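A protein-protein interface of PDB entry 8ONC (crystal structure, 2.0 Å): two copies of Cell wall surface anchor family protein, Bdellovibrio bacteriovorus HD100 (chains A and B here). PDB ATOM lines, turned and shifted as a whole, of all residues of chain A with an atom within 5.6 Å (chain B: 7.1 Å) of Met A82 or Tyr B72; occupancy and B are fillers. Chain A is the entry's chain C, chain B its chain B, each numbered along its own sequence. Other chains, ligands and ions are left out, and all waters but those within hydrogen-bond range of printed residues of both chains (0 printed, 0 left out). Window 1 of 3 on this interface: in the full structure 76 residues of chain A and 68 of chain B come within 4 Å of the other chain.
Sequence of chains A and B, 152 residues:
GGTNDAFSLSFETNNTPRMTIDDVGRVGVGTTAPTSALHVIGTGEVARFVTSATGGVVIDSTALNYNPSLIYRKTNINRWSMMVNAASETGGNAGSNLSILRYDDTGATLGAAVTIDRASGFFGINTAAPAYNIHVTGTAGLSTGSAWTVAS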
ATOM      1  N   VAL A  58      -2.718  22.666 -10.066  1.00  0.00           N
ATOM      2  CA  VAL A  58      -2.569  21.802  -8.901  1.00  0.00           C
ATOM      3  C   VAL A  58      -1.389  22.293  -8.074  1.00  0.00           C
ATOM      4  O   VAL A  58      -0.280  22.455  -8.598  1.00  0.00           O
ATOM      5  CB  VAL A  58      -2.365  20.331  -9.309  1.00  0.00           C
ATOM      6  CG1 VAL A  58      -2.084  19.473  -8.082  1.00  0.00           C
ATOM      7  CG2 VAL A  58      -3.578  19.815 -10.066  1.00  0.00           C
ATOM      8  N   ILE A  59      -1.631  22.530  -6.787  1.00  0.00           N
ATOM      9  CA  ILE A  59      -0.577  22.753  -5.804  1.00  0.00           C
ATOM     10  C   ILE A  59      -0.465  21.482  -4.973  1.00  0.00           C
ATOM     11  O   ILE A  59      -1.427  21.086  -4.302  1.00  0.00           O
ATOM     12  CB  ILE A  59      -0.866  23.973  -4.915  1.00  0.00           C
ATOM     13  CG1 ILE A  59      -1.219  25.189  -5.774  1.00  0.00           C
ATOM     14  CG2 ILE A  59       0.335  24.280  -4.028  1.00  0.00           C
ATOM     15  CD1 ILE A  59      -1.597  26.416  -4.962  1.00  0.00           C
ATOM     16  N   PRO A  68       0.577  22.300   1.283  1.00  0.00           N
ATOM     17  CA  PRO A  68       0.511  23.136   0.077  1.00  0.00           C
ATOM     18  C   PRO A  68      -0.287  24.406   0.327  1.00  0.00           C
ATOM     19  O   PRO A  68      -1.318  24.392   1.004  1.00  0.00           O
ATOM     20  CB  PRO A  68      -0.182  22.226  -0.941  1.00  0.00           C
ATOM     21  CG  PRO A  68      -1.060  21.356  -0.099  1.00  0.00           C
ATOM     22  CD  PRO A  68      -0.282  21.107   1.175  1.00  0.00           C
ATOM     23  N   SER A  69       0.194  25.513  -0.237  1.00  0.00           N
ATOM     24  CA  SER A  69      -0.381  26.812   0.074  1.00  0.00           C
ATOM     25  C   SER A  69      -0.369  27.710  -1.154  1.00  0.00           C
ATOM     26  O   SER A  69       0.511  27.608  -2.015  1.00  0.00           O
ATOM     27  CB  SER A  69       0.380  27.495   1.217  1.00  0.00           C
ATOM     28  OG  SER A  69       1.758  27.614   0.912  1.00  0.00           O
ATOM     29  N   LEU A  70      -1.365  28.589  -1.222  1.00  0.00           N
ATOM     30  CA  LEU A  70      -1.386  29.729  -2.127  1.00  0.00           C
ATOM     31  C   LEU A  70      -1.198  30.980  -1.279  1.00  0.00           C
ATOM     32  O   LEU A  70      -2.002  31.246  -0.379  1.00  0.00           O
ATOM     33  CB  LEU A  70      -2.703  29.796  -2.901  1.00  0.00           C
ATOM     34  CG  LEU A  70      -2.954  31.052  -3.740  1.00  0.00           C
ATOM     35  CD1 LEU A  70      -2.012  31.108  -4.939  1.00  0.00           C
ATOM     36  CD2 LEU A  70      -4.407  31.112  -4.189  1.00  0.00           C
ATOM     37  N   ILE A  71      -0.141  31.739  -1.559  1.00  0.00           N
ATOM     38  CA  ILE A  71       0.253  32.870  -0.728  1.00  0.00           C
ATOM     39  C   ILE A  71       0.157  34.152  -1.547  1.00  0.00           C
ATOM     40  O   ILE A  71       0.717  34.239  -2.647  1.00  0.00           O
ATOM     41  CB  ILE A  71       1.673  32.688  -0.163  1.00  0.00           C
ATOM     42  CG1 ILE A  71       1.692  31.545   0.852  1.00  0.00           C
ATOM     43  CG2 ILE A  71       2.157  33.971   0.492  1.00  0.00           C
ATOM     44  CD1 ILE A  71       3.027  30.844   0.952  1.00  0.00           C
ATOM     45  N   TYR A  72      -0.558  35.138  -1.007  1.00  0.00           N
ATOM     46  CA  TYR A  72      -0.653  36.477  -1.566  1.00  0.00           C
ATOM     47  C   TYR A  72       0.273  37.415  -0.806  1.00  0.00           C
ATOM     48  O   TYR A  72       0.151  37.555   0.423  1.00  0.00           O
ATOM     49  CB  TYR A  72      -2.077  37.025  -1.474  1.00  0.00           C
ATOM     50  CG  TYR A  72      -3.139  36.287  -2.249  1.00  0.00           C
ATOM     51  CD1 TYR A  72      -3.767  35.169  -1.716  1.00  0.00           C
ATOM     52  CD2 TYR A  72      -3.546  36.736  -3.500  1.00  0.00           C
ATOM     53  CE1 TYR A  72      -4.756  34.504  -2.417  1.00  0.00           C
ATOM     54  CE2 TYR A  72      -4.533  36.077  -4.208  1.00  0.00           C
ATOM     55  CZ  TYR A  72      -5.135  34.964  -3.661  1.00  0.00           C
ATOM     56  OH  TYR A  72      -6.119  34.304  -4.359  1.00  0.00           O
ATOM     57  N   TRP A  80      -1.876  37.402   2.726  1.00  0.00           N
ATOM     58  CA  TRP A  80      -2.902  36.392   2.960  1.00  0.00           C
ATOM     59  C   TRP A  80      -2.425  35.047   2.442  1.00  0.00           C
ATOM     60  O   TRP A  80      -1.478  34.965   1.663  1.00  0.00           O
ATOM     61  CB  TRP A  80      -4.238  36.751   2.289  1.00  0.00           C
ATOM     62  CG  TRP A  80      -4.960  37.892   2.926  1.00  0.00           C
ATOM     63  CD1 TRP A  80      -4.810  39.218   2.642  1.00  0.00           C
ATOM     64  CD2 TRP A  80      -5.954  37.811   3.956  1.00  0.00           C
ATOM     65  NE1 TRP A  80      -5.650  39.970   3.433  1.00  0.00           N
ATOM     66  CE2 TRP A  80      -6.361  39.129   4.247  1.00  0.00           C
ATOM     67  CE3 TRP A  80      -6.536  36.752   4.661  1.00  0.00           C
ATOM     68  CZ2 TRP A  80      -7.329  39.415   5.210  1.00  0.00           C
ATOM     69  CZ3 TRP A  80      -7.500  37.042   5.620  1.00  0.00           C
ATOM     70  CH2 TRP A  80      -7.883  38.363   5.885  1.00  0.00           C
ATOM     71  N   SER A  81      -3.090  33.982   2.884  1.00  0.00           N
ATOM     72  CA  SER A  81      -2.808  32.677   2.300  1.00  0.00           C
ATOM     73  C   SER A  81      -4.011  31.764   2.465  1.00  0.00           C
ATOM     74  O   SER A  81      -4.771  31.878   3.427  1.00  0.00           O
ATOM     75  CB  SER A  81      -1.565  32.020   2.919  1.00  0.00           C
ATOM     76  OG  SER A  81      -1.818  31.562   4.234  1.00  0.00           O
ATOM     77  N   MET A  82      -4.180  30.866   1.502  1.00  0.00           N
ATOM     78  CA  MET A  82      -5.130  29.764   1.597  1.00  0.00           C
ATOM     79  C   MET A  82      -4.341  28.469   1.494  1.00  0.00           C
ATOM     80  O   MET A  82      -3.651  28.239   0.494  1.00  0.00           O
ATOM     81  CB  MET A  82      -6.196  29.841   0.503  1.00  0.00           C
ATOM     82  CG  MET A  82      -7.399  28.947   0.763  1.00  0.00           C
ATOM     83  SD  MET A  82      -8.629  28.996  -0.553  1.00  0.00           S
ATOM     84  CE  MET A  82     -10.009  29.745   0.299  1.00  0.00           C
ATOM     85  N   MET A  83      -4.432  27.631   2.522  1.00  0.00           N
ATOM     86  CA  MET A  83      -3.538  26.487   2.602  1.00  0.00           C
ATOM     87  C   MET A  83      -4.254  25.300   3.226  1.00  0.00           C
ATOM     88  O   MET A  83      -5.277  25.443   3.900  1.00  0.00           O
ATOM     89  CB  MET A  83      -2.280  26.833   3.403  1.00  0.00           C
ATOM     90  CG  MET A  83      -2.551  27.153   4.865  1.00  0.00           C
ATOM     91  SD  MET A  83      -1.031  27.290   5.820  1.00  0.00           S
ATOM     92  CE  MET A  83      -0.207  25.773   5.364  1.00  0.00           C
ATOM     93  N   VAL A  84      -3.710  24.118   2.971  1.00  0.00           N
ATOM     94  CA  VAL A  84      -4.127  22.900   3.655  1.00  0.00           C
ATOM     95  C   VAL A  84      -3.209  22.724   4.855  1.00  0.00           C
ATOM     96  O   VAL A  84      -1.992  22.598   4.695  1.00  0.00           O
ATOM     97  CB  VAL A  84      -4.064  21.686   2.719  1.00  0.00           C
ATOM     98  CG1 VAL A  84      -4.517  20.435   3.445  1.00  0.00           C
ATOM     99  CG2 VAL A  84      -4.921  21.926   1.494  1.00  0.00           C
ATOM    100  N   LEU A  98      -8.662  23.055   5.742  1.00  0.00           N
ATOM    101  CA  LEU A  98      -8.383  24.248   4.952  1.00  0.00           C
ATOM    102  C   LEU A  98      -8.357  25.468   5.861  1.00  0.00           C
ATOM    103  O   LEU A  98      -9.223  25.620   6.723  1.00  0.00           O
ATOM    104  CB  LEU A  98      -9.422  24.434   3.844  1.00  0.00           C
ATOM    105  CG  LEU A  98      -9.096  25.519   2.812  1.00  0.00           C
ATOM    106  CD1 LEU A  98      -7.964  25.079   1.881  1.00  0.00           C
ATOM    107  CD2 LEU A  98     -10.336  25.897   2.013  1.00  0.00           C
ATOM    108  N   SER A  99      -7.365  26.333   5.670  1.00  0.00           N
ATOM    109  CA  SER A  99      -7.222  27.530   6.484  1.00  0.00           C
ATOM    110  C   SER A  99      -6.944  28.732   5.597  1.00  0.00           C
ATOM    111  O   SER A  99      -6.163  28.649   4.641  1.00  0.00           O
ATOM    112  CB  SER A  99      -6.092  27.378   7.517  1.00  0.00           C
ATOM    113  OG  SER A  99      -6.549  26.699   8.674  1.00  0.00           O
ATOM    114  N   ILE A 100      -7.595  29.845   5.917  1.00  0.00           N
ATOM    115  CA  ILE A 100      -7.277  31.144   5.334  1.00  0.00           C
ATOM    116  C   ILE A 100      -6.561  31.954   6.407  1.00  0.00           C
ATOM    117  O   ILE A 100      -7.173  32.368   7.400  1.00  0.00           O
ATOM    118  CB  ILE A 100      -8.524  31.877   4.824  1.00  0.00           C
ATOM    119  CG1 ILE A 100      -9.218  31.065   3.732  1.00  0.00           C
ATOM    120  CG2 ILE A 100      -8.149  33.256   4.296  1.00  0.00           C
ATOM    121  CD1 ILE A 100     -10.536  31.672   3.288  1.00  0.00           C
ATOM    122  N   LEU A 101      -5.267  32.181   6.206  1.00  0.00           N
ATOM    123  CA  LEU A 101      -4.419  32.884   7.156  1.00  0.00           C
ATOM    124  C   LEU A 101      -4.252  34.339   6.747  1.00  0.00           C
ATOM    125  O   LEU A 101      -4.139  34.652   5.557  1.00  0.00           O
ATOM    126  CB  LEU A 101      -3.036  32.231   7.241  1.00  0.00           C
ATOM    127  CG  LEU A 101      -2.923  30.730   7.511  1.00  0.00           C
ATOM    128  CD1 LEU A 101      -1.477  30.363   7.797  1.00  0.00           C
ATOM    129  CD2 LEU A 101      -3.805  30.315   8.663  1.00  0.00           C
ATOM    130  N   LEU B  70      -8.615  25.261  -8.894  1.00  0.00           N
ATOM    131  CA  LEU B  70      -7.350  25.237  -8.171  1.00  0.00           C
ATOM    132  C   LEU B  70      -7.448  24.094  -7.169  1.00  0.00           C
ATOM    133  O   LEU B  70      -8.342  24.096  -6.316  1.00  0.00           O
ATOM    134  CB  LEU B  70      -7.090  26.564  -7.459  1.00  0.00           C
ATOM    135  CG  LEU B  70      -5.893  26.581  -6.503  1.00  0.00           C
ATOM    136  CD1 LEU B  70      -4.582  26.448  -7.271  1.00  0.00           C
ATOM    137  CD2 LEU B  70      -5.892  27.827  -5.634  1.00  0.00           C
ATOM    138  N   ILE B  71      -6.555  23.115  -7.284  1.00  0.00           N
ATOM    139  CA  ILE B  71      -6.641  21.876  -6.515  1.00  0.00           C
ATOM    140  C   ILE B  71      -5.434  21.772  -5.593  1.00  0.00           C
ATOM    141  O   ILE B  71      -4.288  21.905  -6.040  1.00  0.00           O
ATOM    142  CB  ILE B  71      -6.727  20.642  -7.433  1.00  0.00           C
ATOM    143  CG1 ILE B  71      -7.951  20.735  -8.343  1.00  0.00           C
ATOM    144  CG2 ILE B  71      -6.769  19.363  -6.614  1.00  0.00           C
ATOM    145  CD1 ILE B  71      -7.886  19.812  -9.548  1.00  0.00           C
ATOM    146  N   TYR B  72      -5.696  21.523  -4.308  1.00  0.00           N
ATOM    147  CA  TYR B  72      -4.675  21.256  -3.306  1.00  0.00           C
ATOM    148  C   TYR B  72      -4.603  19.755  -3.059  1.00  0.00           C
ATOM    149  O   TYR B  72      -5.612  19.140  -2.670  1.00  0.00           O
ATOM    150  CB  TYR B  72      -4.987  21.959  -1.987  1.00  0.00           C
ATOM    151  CG  TYR B  72      -5.018  23.467  -2.020  1.00  0.00           C
ATOM    152  CD1 TYR B  72      -6.163  24.147  -2.409  1.00  0.00           C
ATOM    153  CD2 TYR B  72      -3.921  24.213  -1.606  1.00  0.00           C
ATOM    154  CE1 TYR B  72      -6.208  25.524  -2.416  1.00  0.00           C
ATOM    155  CE2 TYR B  72      -3.955  25.595  -1.612  1.00  0.00           C
ATOM    156  CZ  TYR B  72      -5.103  26.245  -2.015  1.00  0.00           C
ATOM    157  OH  TYR B  72      -5.151  27.619  -2.024  1.00  0.00           O
ATOM    158  N   ARG B  73      -3.402  19.192  -3.235  1.00  0.00           N
ATOM    159  CA  ARG B  73      -3.128  17.775  -3.058  1.00  0.00           C
ATOM    160  C   ARG B  73      -1.965  17.580  -2.092  1.00  0.00           C
ATOM    161  O   ARG B  73      -1.105  18.452  -1.943  1.00  0.00           O
ATOM    162  CB  ARG B  73      -2.775  17.101  -4.396  1.00  0.00           C
ATOM    163  CG  ARG B  73      -3.900  17.083  -5.410  1.00  0.00           C
ATOM    164  CD  ARG B  73      -3.543  16.234  -6.619  1.00  0.00           C
ATOM    165  NE  ARG B  73      -4.596  16.276  -7.626  1.00  0.00           N
ATOM    166  CZ  ARG B  73      -4.408  16.046  -8.918  1.00  0.00           C
ATOM    167  NH1 ARG B  73      -3.212  15.748  -9.402  1.00  0.00           N
ATOM    168  NH2 ARG B  73      -5.445  16.125  -9.748  1.00  0.00           N
ATOM    169  N   LYS B  74      -1.950  16.418  -1.444  1.00  0.00           N
ATOM    170  CA  LYS B  74      -0.804  15.948  -0.674  1.00  0.00           C
ATOM    171  C   LYS B  74      -0.465  14.548  -1.156  1.00  0.00           C
ATOM    172  O   LYS B  74      -1.354  13.698  -1.264  1.00  0.00           O
ATOM    173  CB  LYS B  74      -1.086  15.942   0.833  1.00  0.00           C
ATOM    174  CG  LYS B  74      -1.276  17.317   1.451  1.00  0.00           C
ATOM    175  CD  LYS B  74      -1.581  17.201   2.939  1.00  0.00           C
ATOM    176  CE  LYS B  74      -1.064  18.406   3.710  1.00  0.00           C
ATOM    177  NZ  LYS B  74      -1.345  18.290   5.167  1.00  0.00           N
ATOM    178  N   ILE B  77      -2.711  13.387  -3.897  1.00  0.00           N
ATOM    179  CA  ILE B  77      -4.080  12.975  -3.611  1.00  0.00           C
ATOM    180  C   ILE B  77      -4.889  14.219  -3.273  1.00  0.00           C
ATOM    181  O   ILE B  77      -4.463  15.028  -2.440  1.00  0.00           O
ATOM    182  CB  ILE B  77      -4.149  11.953  -2.462  1.00  0.00           C
ATOM    183  CG1 ILE B  77      -3.179  10.797  -2.711  1.00  0.00           C
ATOM    184  CG2 ILE B  77      -5.569  11.433  -2.299  1.00  0.00           C
ATOM    185  CD1 ILE B  77      -3.074   9.845  -1.542  1.00  0.00           C
ATOM    186  N   ASN B  78      -6.048  14.367  -3.917  1.00  0.00           N
ATOM    187  CA  ASN B  78      -6.896  15.531  -3.691  1.00  0.00           C
ATOM    188  C   ASN B  78      -7.202  15.700  -2.210  1.00  0.00           C
ATOM    189  O   ASN B  78      -7.537  14.737  -1.515  1.00  0.00           O
ATOM    190  CB  ASN B  78      -8.207  15.400  -4.469  1.00  0.00           C
ATOM    191  CG  ASN B  78      -8.015  15.487  -5.970  1.00  0.00           C
ATOM    192  OD1 ASN B  78      -7.005  15.992  -6.453  1.00  0.00           O
ATOM    193  ND2 ASN B  78      -8.992  14.991  -6.716  1.00  0.00           N
ATOM    194  N   ARG B  79      -7.080  16.932  -1.733  1.00  0.00           N
ATOM    195  CA  ARG B  79      -7.535  17.290  -0.397  1.00  0.00           C
ATOM    196  C   ARG B  79      -8.551  18.417  -0.430  1.00  0.00           C
ATOM    197  O   ARG B  79      -9.600  18.318   0.219  1.00  0.00           O
ATOM    198  CB  ARG B  79      -6.341  17.672   0.493  1.00  0.00           C
ATOM    199  CG  ARG B  79      -5.433  16.499   0.820  1.00  0.00           C
ATOM    200  CD  ARG B  79      -6.094  15.599   1.847  1.00  0.00           C
ATOM    201  NE  ARG B  79      -5.278  14.444   2.201  1.00  0.00           N
ATOM    202  CZ  ARG B  79      -5.385  13.255   1.625  1.00  0.00           C
ATOM    203  NH1 ARG B  79      -6.232  13.042   0.631  1.00  0.00           N
ATOM    204  NH2 ARG B  79      -4.623  12.253   2.057  1.00  0.00           N
ATOM    205  N   TRP B  80      -8.283  19.483  -1.180  1.00  0.00           N
ATOM    206  CA  TRP B  80      -9.241  20.578  -1.262  1.00  0.00           C
ATOM    207  C   TRP B  80      -9.230  21.147  -2.669  1.00  0.00           C
ATOM    208  O   TRP B  80      -8.311  20.898  -3.446  1.00  0.00           O
ATOM    209  CB  TRP B  80      -8.935  21.692  -0.254  1.00  0.00           C
ATOM    210  CG  TRP B  80      -9.202  21.341   1.174  1.00  0.00           C
ATOM    211  CD1 TRP B  80      -8.330  20.777   2.060  1.00  0.00           C
ATOM    212  CD2 TRP B  80     -10.423  21.550   1.891  1.00  0.00           C
ATOM    213  NE1 TRP B  80      -8.935  20.619   3.285  1.00  0.00           N
ATOM    214  CE2 TRP B  80     -10.222  21.084   3.207  1.00  0.00           C
ATOM    215  CE3 TRP B  80     -11.671  22.083   1.547  1.00  0.00           C
ATOM    216  CZ2 TRP B  80     -11.220  21.137   4.179  1.00  0.00           C
ATOM    217  CZ3 TRP B  80     -12.662  22.134   2.516  1.00  0.00           C
ATOM    218  CH2 TRP B  80     -12.429  21.661   3.814  1.00  0.00           C
ATOM    219  N   SER B  81     -10.260  21.920  -2.998  1.00  0.00           N
ATOM    220  CA  SER B  81     -10.221  22.650  -4.258  1.00  0.00           C
ATOM    221  C   SER B  81     -11.127  23.867  -4.180  1.00  0.00           C
ATOM    222  O   SER B  81     -12.120  23.875  -3.451  1.00  0.00           O
ATOM    223  CB  SER B  81     -10.621  21.768  -5.452  1.00  0.00           C
ATOM    224  OG  SER B  81     -11.991  21.413  -5.406  1.00  0.00           O
ATOM    225  N   MET B  82     -10.758  24.903  -4.925  1.00  0.00           N
ATOM    226  CA  MET B  82     -11.621  26.054  -5.163  1.00  0.00           C
ATOM    227  C   MET B  82     -11.851  26.158  -6.663  1.00  0.00           C
ATOM    228  O   MET B  82     -10.892  26.269  -7.435  1.00  0.00           O
ATOM    229  CB  MET B  82     -11.014  27.344  -4.611  1.00  0.00           C
ATOM    230  CG  MET B  82     -11.982  28.522  -4.645  1.00  0.00           C
ATOM    231  SD  MET B  82     -11.278  30.074  -4.056  1.00  0.00           S
ATOM    232  CE  MET B  82     -12.193  30.313  -2.538  1.00  0.00           C
ATOM    233  N   ILE B 100     -15.946  25.586  -2.833  1.00  0.00           N
ATOM    234  CA  ILE B 100     -14.817  25.001  -2.126  1.00  0.00           C
ATOM    235  C   ILE B 100     -15.182  23.557  -1.811  1.00  0.00           C
ATOM    236  O   ILE B 100     -16.095  23.292  -1.019  1.00  0.00           O
ATOM    237  CB  ILE B 100     -14.463  25.788  -0.860  1.00  0.00           C
ATOM    238  CG1 ILE B 100     -14.119  27.234  -1.228  1.00  0.00           C
ATOM    239  CG2 ILE B 100     -13.301  25.128  -0.146  1.00  0.00           C
ATOM    240  CD1 ILE B 100     -13.779  28.101  -0.037  1.00  0.00           C
ATOM    241  N   TYR B 103     -12.183  16.666  -0.027  1.00  0.00           N
ATOM    242  CA  TYR B 103     -11.978  15.318  -0.538  1.00  0.00           C
ATOM    243  C   TYR B 103     -11.528  14.403   0.590  1.00  0.00           C
ATOM    244  O   TYR B 103     -10.886  14.844   1.548  1.00  0.00           O
ATOM    245  CB  TYR B 103     -10.939  15.305  -1.670  1.00  0.00           C
ATOM    246  CG  TYR B 103     -11.319  16.181  -2.843  1.00  0.00           C
ATOM    247  CD1 TYR B 103     -11.066  17.548  -2.822  1.00  0.00           C
ATOM    248  CD2 TYR B 103     -11.937  15.646  -3.966  1.00  0.00           C
ATOM    249  CE1 TYR B 103     -11.414  18.354  -3.886  1.00  0.00           C
ATOM    250  CE2 TYR B 103     -12.291  16.445  -5.035  1.00  0.00           C
ATOM    251  CZ  TYR B 103     -12.026  17.797  -4.990  1.00  0.00           C
ATOM    252  OH  TYR B 103     -12.373  18.597  -6.051  1.00  0.00           O
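O of Ile B71 touches CA of Val A58 (3.3 Å).
Arg B73 touches Val A58.
Ile A59 touches Tyr B72 (O to CA, 3.4 Å).
Arg B73 touches Pro A68 (O to CG, 3.4 Å).
CE of Lys B74 touches CD of Pro A68 (3.8 Å).
Leu B70 touches Leu A70 (CD2 to CD2, 3.9 Å).
Leu A70 touches Tyr B72.
Val A84 touches Tyr B72 (CG2 to CB, 3.5 Å).
Val A84 touches Trp B80.
CG2 of Ile B100 touches CD2 of Leu A98, at 3.7 Å.
Of the 16 printed residues of chain A, 7 touch a printed residue of chain B.
Printed residues of chain A that touch a printed residue of chain B: Val A58, Ile A59, Pro A68, Leu A70, Met A82, Val A84 and Leu A98.
Hydrophobic or aromatic side chains of chain A that line the printed part of chain B: Val A58, Ile A59, Pro A68, Leu A70, Met A82, Val A84 and Leu A98.
Of the 13 printed residues of chain B, 8 touch a printed residue of chain A.
Hydrophobic or aromatic side chains of chain B within 4 Å of the printed part of chain A: Leu B70, Tyr B72, Trp B80, Met B82 and Ile B100.
Among the printed residues, 17 pairs touch across the chains.
Among the printed residues, no Asp or Glu carboxylate lies within 4 Å of a Lys or Arg side-chain nitrogen of the other chain.
O of Ile B71 is in hydrogen-bond range of N of Ile A59 (2.8 Å).
The backbone NH (N) of Arg B73 sits at hydrogen-bond distance from the backbone carbonyl oxygen (O) of Ile A59 (2.9 Å).
OH of Tyr B72 sits at hydrogen-bond distance from O of Met A82 (3.0 Å).
The backbone NH (N) of Leu A98 sits close to the indole nitrogen (NE1) of Trp B80, at 3.5 Å.
Of the printed residues of chain B, Ile A59 touches Leu B70 (3.8 Å), Ile B71 (2.8 Å), Tyr B72 (3.4 Å) and Arg B73 (2.9 Å).
Ser A69 touches none of the printed residues of chain B.
Of the printed residues of chain B, Leu A70 touches Leu B70 and Tyr B72.
Tyr A72 touches none of the printed residues of chain B.
Met A82 touches just these residues of chain B: Tyr B72 (3.0 Å) and Met B82 (3.6 Å).
Tyr B72 touches five residues of chain A.
Printed residues of chain A within 4 Å of Met B82: Met A82 (3.6 Å).
The nearest residue of chain A that does not touch Tyr B72 is Ser A69 (4.1 Å).
Leu A70 touches its own counterpart, Leu B70.
Leu A70 touches Tyr B72, but with the chains exchanged Tyr A72 does not touch Leu B70 (6.6 Å).
Met A82 touches Tyr B72, but with the chains exchanged Tyr A72 does not touch Met B82 (6.7 Å).
Met B82 touches its own counterpart, Met A82.
Positions printed for both chains: 70, 71, 72, 80, 81, 82 and 100.
O of Pro A68 lies within hydrogen-bond range of N of Val A84, at 3.1 Å.
The backbone NH (N) of Leu A70 sits at hydrogen-bond distance from the backbone carbonyl oxygen (O) of Met A82 (2.9 Å).
N of Leu B70 lies within hydrogen-bond range of O of Met B82 (2.9 Å).
The backbone carbonyl oxygen of Tyr B72 sits at hydrogen-bond distance from the backbone NH of Arg B79, 2.8 Å away.
The backbone NH of Tyr B72 is in hydrogen-bond range of the backbone carbonyl oxygen of Trp B80, 2.8 Å away.
OD1 of Asn B78 lies within hydrogen-bond range of NE of Arg B73.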
